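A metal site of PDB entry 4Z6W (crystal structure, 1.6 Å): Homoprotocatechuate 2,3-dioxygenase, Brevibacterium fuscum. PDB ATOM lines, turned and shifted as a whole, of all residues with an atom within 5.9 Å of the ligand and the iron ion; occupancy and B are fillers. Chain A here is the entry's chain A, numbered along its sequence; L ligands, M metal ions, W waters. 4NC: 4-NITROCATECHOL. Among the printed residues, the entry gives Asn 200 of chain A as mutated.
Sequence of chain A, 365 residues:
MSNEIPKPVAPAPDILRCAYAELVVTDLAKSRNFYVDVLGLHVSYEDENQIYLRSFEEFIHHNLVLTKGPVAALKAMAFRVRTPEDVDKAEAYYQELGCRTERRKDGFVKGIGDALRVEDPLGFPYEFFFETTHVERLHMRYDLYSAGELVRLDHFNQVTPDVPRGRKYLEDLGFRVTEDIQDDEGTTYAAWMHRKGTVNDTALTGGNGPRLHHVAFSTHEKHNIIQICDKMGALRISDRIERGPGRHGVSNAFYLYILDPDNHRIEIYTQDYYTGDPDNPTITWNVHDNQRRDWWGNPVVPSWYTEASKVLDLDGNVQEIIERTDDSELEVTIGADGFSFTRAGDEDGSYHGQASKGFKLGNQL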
ATOM      1  N   HIS A 155       1.099 -26.844 -33.382  1.00  0.00           N
ATOM      2  CA  HIS A 155      -0.110 -26.693 -34.227  1.00  0.00           C
ATOM      3  C   HIS A 155      -0.519 -25.272 -34.466  1.00  0.00           C
ATOM      4  O   HIS A 155      -0.049 -24.355 -33.811  1.00  0.00           O
ATOM      5  CB  HIS A 155      -1.290 -27.498 -33.631  1.00  0.00           C
ATOM      6  CG  HIS A 155      -1.813 -27.007 -32.311  1.00  0.00           C
ATOM      7  ND1 HIS A 155      -1.426 -27.538 -31.108  1.00  0.00           N
ATOM      8  CD2 HIS A 155      -2.752 -26.071 -32.020  1.00  0.00           C
ATOM      9  CE1 HIS A 155      -2.111 -26.966 -30.119  1.00  0.00           C
ATOM     10  NE2 HIS A 155      -2.896 -26.054 -30.648  1.00  0.00           N
ATOM     11  N   PHE A 156      -1.454 -25.148 -35.386  1.00  0.00           N
ATOM     12  CA  PHE A 156      -2.206 -23.938 -35.628  1.00  0.00           C
ATOM     13  C   PHE A 156      -3.670 -24.155 -35.227  1.00  0.00           C
ATOM     14  O   PHE A 156      -4.139 -25.300 -35.175  1.00  0.00           O
ATOM     15  CB  PHE A 156      -2.194 -23.603 -37.126  1.00  0.00           C
ATOM     16  CG  PHE A 156      -0.824 -23.615 -37.768  1.00  0.00           C
ATOM     17  CD1 PHE A 156       0.230 -22.864 -37.232  1.00  0.00           C
ATOM     18  CD2 PHE A 156      -0.613 -24.345 -38.937  1.00  0.00           C
ATOM     19  CE1 PHE A 156       1.482 -22.856 -37.855  1.00  0.00           C
ATOM     20  CE2 PHE A 156       0.635 -24.348 -39.551  1.00  0.00           C
ATOM     21  CZ  PHE A 156       1.667 -23.604 -39.023  1.00  0.00           C
ATOM     22  N   ASN A 157      -4.399 -23.067 -35.030  1.00  0.00           N
ATOM     23  CA  ASN A 157      -5.860 -23.166 -34.831  1.00  0.00           C
ATOM     24  C   ASN A 157      -6.507 -21.982 -35.568  1.00  0.00           C
ATOM     25  O   ASN A 157      -6.150 -20.840 -35.349  1.00  0.00           O
ATOM     26  CB  ASN A 157      -6.178 -23.123 -33.330  1.00  0.00           C
ATOM     27  CG  ASN A 157      -7.639 -23.359 -33.043  1.00  0.00           C
ATOM     28  OD1 ASN A 157      -8.486 -22.632 -33.524  1.00  0.00           O
ATOM     29  ND2 ASN A 157      -7.936 -24.380 -32.231  1.00  0.00           N
ATOM     30  N   ILE A 181     -16.175 -30.944 -30.974  1.00  0.00           N
ATOM     31  CA  ILE A 181     -17.191 -30.483 -30.058  1.00  0.00           C
ATOM     32  C   ILE A 181     -18.479 -30.265 -30.843  1.00  0.00           C
ATOM     33  O   ILE A 181     -18.497 -29.543 -31.858  1.00  0.00           O
ATOM     34  CB  ILE A 181     -16.777 -29.179 -29.360  1.00  0.00           C
ATOM     35  CG1 ILE A 181     -15.547 -29.379 -28.449  1.00  0.00           C
ATOM     36  CG2 ILE A 181     -17.939 -28.622 -28.541  1.00  0.00           C
ATOM     37  CD1 ILE A 181     -14.950 -28.091 -27.876  1.00  0.00           C
ATOM     38  N   TRP A 192     -10.446 -30.833 -34.370  1.00  0.00           N
ATOM     39  CA  TRP A 192      -9.007 -30.937 -34.363  1.00  0.00           C
ATOM     40  C   TRP A 192      -8.581 -32.024 -35.308  1.00  0.00           C
ATOM     41  O   TRP A 192      -9.189 -33.097 -35.332  1.00  0.00           O
ATOM     42  CB  TRP A 192      -8.520 -31.253 -32.958  1.00  0.00           C
ATOM     43  CG  TRP A 192      -8.609 -30.080 -31.958  1.00  0.00           C
ATOM     44  CD1 TRP A 192      -7.583 -29.264 -31.554  1.00  0.00           C
ATOM     45  CD2 TRP A 192      -9.783 -29.593 -31.301  1.00  0.00           C
ATOM     46  NE1 TRP A 192      -8.048 -28.309 -30.696  1.00  0.00           N
ATOM     47  CE2 TRP A 192      -9.393 -28.481 -30.524  1.00  0.00           C
ATOM     48  CE3 TRP A 192     -11.123 -29.993 -31.278  1.00  0.00           C
ATOM     49  CZ2 TRP A 192     -10.289 -27.780 -29.712  1.00  0.00           C
ATOM     50  CZ3 TRP A 192     -12.026 -29.268 -30.486  1.00  0.00           C
ATOM     51  CH2 TRP A 192     -11.590 -28.183 -29.711  1.00  0.00           C
ATOM     52  N   VAL A 199      -2.495 -34.771 -31.446  1.00  0.00           N
ATOM     53  CA  VAL A 199      -3.925 -34.436 -31.527  1.00  0.00           C
ATOM     54  C   VAL A 199      -4.231 -33.466 -32.689  1.00  0.00           C
ATOM     55  O   VAL A 199      -5.292 -33.581 -33.284  1.00  0.00           O
ATOM     56  CB  VAL A 199      -4.425 -33.923 -30.146  1.00  0.00           C
ATOM     57  CG1 VAL A 199      -5.840 -33.357 -30.250  1.00  0.00           C
ATOM     58  CG2 VAL A 199      -4.444 -35.092 -29.218  1.00  0.00           C
ATOM     59  N   ASN A 200      -3.279 -32.595 -33.060  1.00  0.00           N
ATOM     60  CA  ASN A 200      -3.558 -31.468 -33.974  1.00  0.00           C
ATOM     61  C   ASN A 200      -2.291 -31.100 -34.752  1.00  0.00           C
ATOM     62  O   ASN A 200      -1.196 -31.040 -34.163  1.00  0.00           O
ATOM     63  CB  ASN A 200      -4.078 -30.263 -33.181  1.00  0.00           C
ATOM     64  CG  ASN A 200      -4.825 -29.259 -34.044  1.00  0.00           C
ATOM     65  OD1 ASN A 200      -4.722 -28.059 -33.854  1.00  0.00           O
ATOM     66  ND2 ASN A 200      -5.540 -29.763 -35.009  1.00  0.00           N
ATOM     67  N   HIS A 213      -6.702 -18.231 -34.861  1.00  0.00           N
ATOM     68  CA  HIS A 213      -6.925 -18.236 -33.447  1.00  0.00           C
ATOM     69  C   HIS A 213      -5.605 -18.226 -32.668  1.00  0.00           C
ATOM     70  O   HIS A 213      -5.433 -17.377 -31.834  1.00  0.00           O
ATOM     71  CB  HIS A 213      -7.811 -19.407 -33.008  1.00  0.00           C
ATOM     72  CG  HIS A 213      -8.387 -19.188 -31.659  1.00  0.00           C
ATOM     73  ND1 HIS A 213      -7.638 -19.373 -30.525  1.00  0.00           N
ATOM     74  CD2 HIS A 213      -9.567 -18.672 -31.247  1.00  0.00           C
ATOM     75  CE1 HIS A 213      -8.349 -19.046 -29.464  1.00  0.00           C
ATOM     76  NE2 HIS A 213      -9.513 -18.585 -29.876  1.00  0.00           N
ATOM     77  N   HIS A 214      -4.722 -19.189 -32.925  1.00  0.00           N
ATOM     78  CA  HIS A 214      -3.425 -19.211 -32.289  1.00  0.00           C
ATOM     79  C   HIS A 214      -2.459 -20.093 -33.000  1.00  0.00           C
ATOM     80  O   HIS A 214      -2.838 -20.847 -33.879  1.00  0.00           O
ATOM     81  CB  HIS A 214      -3.576 -19.630 -30.804  1.00  0.00           C
ATOM     82  CG  HIS A 214      -4.159 -21.007 -30.588  1.00  0.00           C
ATOM     83  ND1 HIS A 214      -5.502 -21.213 -30.387  1.00  0.00           N
ATOM     84  CD2 HIS A 214      -3.589 -22.221 -30.476  1.00  0.00           C
ATOM     85  CE1 HIS A 214      -5.747 -22.486 -30.184  1.00  0.00           C
ATOM     86  NE2 HIS A 214      -4.600 -23.130 -30.257  1.00  0.00           N
ATOM     87  N   ALA A 216       0.602 -22.721 -31.563  1.00  0.00           N
ATOM     88  CA  ALA A 216       0.949 -23.401 -30.341  1.00  0.00           C
ATOM     89  C   ALA A 216       2.364 -23.947 -30.410  1.00  0.00           C
ATOM     90  O   ALA A 216       2.741 -24.625 -31.397  1.00  0.00           O
ATOM     91  CB  ALA A 216       0.009 -24.567 -30.115  1.00  0.00           C
ATOM     92  N   ARG A 243      -5.599 -16.847 -20.656  1.00  0.00           N
ATOM     93  CA  ARG A 243      -6.369 -18.013 -20.205  1.00  0.00           C
ATOM     94  C   ARG A 243      -5.375 -19.087 -19.783  1.00  0.00           C
ATOM     95  O   ARG A 243      -4.409 -19.365 -20.475  1.00  0.00           O
ATOM     96  CB  ARG A 243      -7.306 -18.506 -21.301  1.00  0.00           C
ATOM     97  CG  ARG A 243      -7.931 -19.875 -21.093  1.00  0.00           C
ATOM     98  CD  ARG A 243      -9.048 -20.242 -22.078  1.00  0.00           C
ATOM     99  NE  ARG A 243      -9.329 -21.644 -21.782  1.00  0.00           N
ATOM    100  CZ  ARG A 243      -9.450 -22.618 -22.666  1.00  0.00           C
ATOM    101  NH1 ARG A 243      -9.540 -22.410 -23.958  1.00  0.00           N
ATOM    102  NH2 ARG A 243      -9.558 -23.847 -22.210  1.00  0.00           N
ATOM    103  N   HIS A 248      -6.474 -29.216 -20.671  1.00  0.00           N
ATOM    104  CA  HIS A 248      -7.562 -29.262 -21.622  1.00  0.00           C
ATOM    105  C   HIS A 248      -8.374 -30.557 -21.429  1.00  0.00           C
ATOM    106  O   HIS A 248      -7.794 -31.604 -21.040  1.00  0.00           O
ATOM    107  CB  HIS A 248      -7.042 -29.310 -23.075  1.00  0.00           C
ATOM    108  CG  HIS A 248      -6.599 -27.998 -23.618  1.00  0.00           C
ATOM    109  ND1 HIS A 248      -7.382 -26.877 -23.566  1.00  0.00           N
ATOM    110  CD2 HIS A 248      -5.486 -27.657 -24.312  1.00  0.00           C
ATOM    111  CE1 HIS A 248      -6.767 -25.884 -24.191  1.00  0.00           C
ATOM    112  NE2 HIS A 248      -5.618 -26.335 -24.644  1.00  0.00           N
ATOM    113  N   GLY A 249      -9.662 -30.531 -21.731  1.00  0.00           N
ATOM    114  CA  GLY A 249     -10.394 -31.772 -21.970  1.00  0.00           C
ATOM    115  C   GLY A 249     -10.034 -32.330 -23.316  1.00  0.00           C
ATOM    116  O   GLY A 249      -9.348 -33.324 -23.384  1.00  0.00           O
ATOM    117  N   VAL A 250     -10.506 -31.685 -24.381  1.00  0.00           N
ATOM    118  CA  VAL A 250     -10.059 -31.995 -25.723  1.00  0.00           C
ATOM    119  C   VAL A 250      -8.512 -31.952 -25.744  1.00  0.00           C
ATOM    120  O   VAL A 250      -7.933 -30.977 -25.329  1.00  0.00           O
ATOM    121  CB  VAL A 250     -10.565 -30.944 -26.723  1.00  0.00           C
ATOM    122  CG1 VAL A 250      -9.865 -31.124 -28.062  1.00  0.00           C
ATOM    123  CG2 VAL A 250     -12.088 -31.004 -26.921  1.00  0.00           C
ATOM    124  N   SER A 251      -7.894 -33.047 -26.172  1.00  0.00           N
ATOM    125  CA  SER A 251      -6.425 -33.189 -26.327  1.00  0.00           C
ATOM    126  C   SER A 251      -5.716 -33.679 -25.072  1.00  0.00           C
ATOM    127  O   SER A 251      -4.619 -34.230 -25.171  1.00  0.00           O
ATOM    128  CB  SER A 251      -5.702 -31.917 -26.842  1.00  0.00           C
ATOM    129  OG  SER A 251      -5.389 -31.044 -25.765  1.00  0.00           O
ATOM    130  N   TYR A 257      -2.509 -19.802 -22.595  1.00  0.00           N
ATOM    131  CA  TYR A 257      -2.658 -18.840 -23.746  1.00  0.00           C
ATOM    132  C   TYR A 257      -2.190 -17.457 -23.321  1.00  0.00           C
ATOM    133  O   TYR A 257      -2.639 -16.927 -22.304  1.00  0.00           O
ATOM    134  CB  TYR A 257      -4.109 -18.729 -24.213  1.00  0.00           C
ATOM    135  CG  TYR A 257      -4.702 -19.998 -24.750  1.00  0.00           C
ATOM    136  CD1 TYR A 257      -4.525 -20.386 -26.073  1.00  0.00           C
ATOM    137  CD2 TYR A 257      -5.397 -20.840 -23.928  1.00  0.00           C
ATOM    138  CE1 TYR A 257      -5.035 -21.587 -26.547  1.00  0.00           C
ATOM    139  CE2 TYR A 257      -5.926 -22.031 -24.410  1.00  0.00           C
ATOM    140  CZ  TYR A 257      -5.746 -22.383 -25.711  1.00  0.00           C
ATOM    141  OH  TYR A 257      -6.325 -23.531 -26.152  1.00  0.00           O
ATOM    142  N   GLU A 267      -0.360 -20.258 -27.887  1.00  0.00           N
ATOM    143  CA  GLU A 267      -0.558 -21.327 -26.916  1.00  0.00           C
ATOM    144  C   GLU A 267       0.751 -22.012 -26.575  1.00  0.00           C
ATOM    145  O   GLU A 267       1.574 -22.270 -27.456  1.00  0.00           O
ATOM    146  CB  GLU A 267      -1.520 -22.375 -27.438  1.00  0.00           C
ATOM    147  CG  GLU A 267      -2.011 -23.372 -26.391  1.00  0.00           C
ATOM    148  CD  GLU A 267      -2.941 -24.439 -26.909  1.00  0.00           C
ATOM    149  OE1 GLU A 267      -3.140 -24.529 -28.139  1.00  0.00           O
ATOM    150  OE2 GLU A 267      -3.534 -25.166 -26.077  1.00  0.00           O
ATOM    151  N   TYR A 269       1.846 -25.632 -24.770  1.00  0.00           N
ATOM    152  CA  TYR A 269       1.085 -26.888 -24.841  1.00  0.00           C
ATOM    153  C   TYR A 269       2.001 -28.052 -24.529  1.00  0.00           C
ATOM    154  O   TYR A 269       3.187 -28.066 -24.940  1.00  0.00           O
ATOM    155  CB  TYR A 269       0.530 -26.995 -26.260  1.00  0.00           C
ATOM    156  CG  TYR A 269      -0.359 -28.117 -26.666  1.00  0.00           C
ATOM    157  CD1 TYR A 269      -1.748 -28.003 -26.615  1.00  0.00           C
ATOM    158  CD2 TYR A 269       0.200 -29.255 -27.254  1.00  0.00           C
ATOM    159  CE1 TYR A 269      -2.548 -28.996 -27.125  1.00  0.00           C
ATOM    160  CE2 TYR A 269      -0.602 -30.270 -27.734  1.00  0.00           C
ATOM    161  CZ  TYR A 269      -1.979 -30.122 -27.672  1.00  0.00           C
ATOM    162  OH  TYR A 269      -2.761 -31.097 -28.210  1.00  0.00           O
ATOM    163  N   ARG A 292     -14.871 -29.778 -21.037  1.00  0.00           N
ATOM    164  CA  ARG A 292     -14.378 -30.051 -22.395  1.00  0.00           C
ATOM    165  C   ARG A 292     -13.179 -29.187 -22.793  1.00  0.00           C
ATOM    166  O   ARG A 292     -12.308 -29.648 -23.531  1.00  0.00           O
ATOM    167  CB  ARG A 292     -15.525 -29.828 -23.402  1.00  0.00           C
ATOM    168  CG  ARG A 292     -15.772 -28.375 -23.728  1.00  0.00           C
ATOM    169  CD  ARG A 292     -17.084 -28.096 -24.474  1.00  0.00           C
ATOM    170  NE  ARG A 292     -17.188 -26.667 -24.686  1.00  0.00           N
ATOM    171  CZ  ARG A 292     -17.447 -25.761 -23.728  1.00  0.00           C
ATOM    172  NH1 ARG A 292     -17.702 -26.147 -22.468  1.00  0.00           N
ATOM    173  NH2 ARG A 292     -17.384 -24.472 -24.002  1.00  0.00           N
ATOM    174  N   ARG A 293     -13.120 -27.939 -22.332  1.00  0.00           N
ATOM    175  CA  ARG A 293     -12.036 -27.033 -22.742  1.00  0.00           C
ATOM    176  C   ARG A 293     -11.012 -26.899 -21.630  1.00  0.00           C
ATOM    177  O   ARG A 293      -9.824 -26.923 -21.879  1.00  0.00           O
ATOM    178  CB  ARG A 293     -12.583 -25.688 -23.181  1.00  0.00           C
ATOM    179  CG  ARG A 293     -13.282 -25.755 -24.533  1.00  0.00           C
ATOM    180  CD  ARG A 293     -13.290 -24.439 -25.246  1.00  0.00           C
ATOM    181  NE  ARG A 293     -13.854 -24.543 -26.617  1.00  0.00           N
ATOM    182  CZ  ARG A 293     -13.165 -24.796 -27.713  1.00  0.00           C
ATOM    183  NH1 ARG A 293     -11.854 -25.014 -27.693  1.00  0.00           N
ATOM    184  NH2 ARG A 293     -13.786 -24.757 -28.866  1.00  0.00           N
ATOM    185  N   ASP A 294     -11.492 -26.673 -20.429  1.00  0.00           N
ATOM    186  CA  ASP A 294     -10.664 -26.800 -19.224  1.00  0.00           C
ATOM    187  C   ASP A 294     -11.233 -27.910 -18.385  1.00  0.00           C
ATOM    188  O   ASP A 294     -12.389 -27.846 -17.922  1.00  0.00           O
ATOM    189  CB  ASP A 294     -10.672 -25.512 -18.407  1.00  0.00           C
ATOM    190  CG  ASP A 294      -9.627 -25.531 -17.299  1.00  0.00           C
ATOM    191  OD1 ASP A 294      -8.423 -25.278 -17.607  1.00  0.00           O
ATOM    192  OD2 ASP A 294     -10.008 -25.859 -16.129  1.00  0.00           O
ATOM    193  N   TRP A 304     -11.390 -15.179 -25.461  1.00  0.00           N
ATOM    194  CA  TRP A 304     -10.838 -16.355 -26.122  1.00  0.00           C
ATOM    195  C   TRP A 304     -11.745 -16.768 -27.258  1.00  0.00           C
ATOM    196  O   TRP A 304     -11.302 -17.338 -28.281  1.00  0.00           O
ATOM    197  CB  TRP A 304     -10.625 -17.453 -25.065  1.00  0.00           C
ATOM    198  CG  TRP A 304      -9.760 -18.573 -25.543  1.00  0.00           C
ATOM    199  CD1 TRP A 304      -8.424 -18.643 -25.424  1.00  0.00           C
ATOM    200  CD2 TRP A 304     -10.175 -19.701 -26.282  1.00  0.00           C
ATOM    201  NE1 TRP A 304      -7.971 -19.793 -26.005  1.00  0.00           N
ATOM    202  CE2 TRP A 304      -9.026 -20.457 -26.561  1.00  0.00           C
ATOM    203  CE3 TRP A 304     -11.409 -20.157 -26.755  1.00  0.00           C
ATOM    204  CZ2 TRP A 304      -9.057 -21.643 -27.294  1.00  0.00           C
ATOM    205  CZ3 TRP A 304     -11.441 -21.331 -27.473  1.00  0.00           C
ATOM    206  CH2 TRP A 304     -10.267 -22.045 -27.759  1.00  0.00           C
HETATM  207  C1  4NC L   1      -6.140 -27.041 -28.111  1.00  0.00           C
HETATM  208  C2  4NC L   1      -6.822 -25.759 -27.957  1.00  0.00           C
HETATM  209  C3  4NC L   1      -8.087 -25.700 -27.351  1.00  0.00           C
HETATM  210  C4  4NC L   1      -8.572 -26.864 -26.738  1.00  0.00           C
HETATM  211  C5  4NC L   1      -7.938 -28.082 -26.882  1.00  0.00           C
HETATM  212  C6  4NC L   1      -6.770 -28.209 -27.590  1.00  0.00           C
HETATM  213  O7  4NC L   1      -4.920 -27.088 -28.664  1.00  0.00           O
HETATM  214  O8  4NC L   1      -6.282 -24.624 -28.350  1.00  0.00           O
HETATM  215  N9  4NC L   1      -9.661 -26.758 -25.893  1.00  0.00           N
HETATM  216  O10 4NC L   1     -10.037 -27.852 -25.205  1.00  0.00           O
HETATM  217  O11 4NC L   1      -9.987 -25.538 -25.288  1.00  0.00           O
HETATM  218 FE    FE M   1      -4.525 -25.194 -29.455  1.00  0.00          FE
HETATM  219  O   HOH W   1      -4.552 -29.470 -29.824  1.00  0.00           O
HETATM  220  O   HOH W   2      -5.915 -26.080 -31.277  1.00  0.00           O
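Water W2 lies within hydrogen-bond range of ND2 of Asn 157 (2.8 Å), NE1 of Trp 192 (3.1 Å) and OD1 of Asn 200 (3.5 Å).
The backbone carbonyl oxygen of Arg 292 sits close to an oxygen (O10) of the ligand (3.3 Å).
NE1 of Trp 192 touches C6 of the ligand (3.4 Å).
O of Val 250 touches C5 of the ligand, at 3.3 Å.
OG of Ser 251 touches C6 of the ligand, at 3.6 Å.
Tyr 269 touches the ligand.
Hydrophobic or aromatic side chains within 4 Å of the ligand: His 155, Trp 192, His 214, His 248, Val 250, Tyr 257 and Tyr 269.
Of the 22 residues printed, 12 come within 4 Å of the ligand.
The nearest printed residue that does not touch the ligand is Trp 304 (4.2 Å).
OH of Tyr 257 lies close to O8 of the ligand (2.5 Å).
NH1 of Arg 293 is in hydrogen-bond range of O11 of the ligand, 3.1 Å away.
A ring nitrogen (ND1) of His 248 is in hydrogen-bond range of an oxygen (O10) of the ligand (3.3 Å).
NH1 of Arg 243 lies within hydrogen-bond range of O11 of the ligand (3.4 Å).
OH of Tyr 257 sits at hydrogen-bond distance from OE2 of Glu 267 (3.2 Å).
The backbone carbonyl oxygen (O) of His 155 is in hydrogen-bond range of the backbone NH (N) of Ala 216 (2.9 Å).
O of His 214 lies within hydrogen-bond range of N of Asn 157, 2.9 Å away.
A ring nitrogen (ND1) of His 214 sits at hydrogen-bond distance from a ring nitrogen (ND1) of His 213, at 2.8 Å.
The backbone NH (N) of Tyr 257 lies within hydrogen-bond range of the backbone carbonyl oxygen (O) of Arg 243 (2.9 Å).
ND1 of His 248 is in hydrogen-bond range of O of Arg 293, at 3.0 Å.
The backbone carbonyl oxygen (O) of Arg 293 lies within hydrogen-bond range of the guanidinium group (NH2) of Arg 243, 3.1 Å away.
The backbone carbonyl oxygen (O) of Arg 292 lies within hydrogen-bond range of the backbone NH (N) of Val 250 (2.8 Å).
Three residues have an atom within 4 Å of the iron ion: His 155, His 214 and Glu 267.
Along chain A the residues within 4 Å of the iron ion span positions 155 to 267.
The iron ion is bound by OE1 of Glu 267 (2.0 Å), O7 of the ligand (2.1 Å), O8 of the ligand (2.2 Å), NE2 of His 155 (2.2 Å), NE2 of His 214 (2.2 Å) and water W2 (2.5 Å).
The iron ion has six donor atoms within binding distance.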
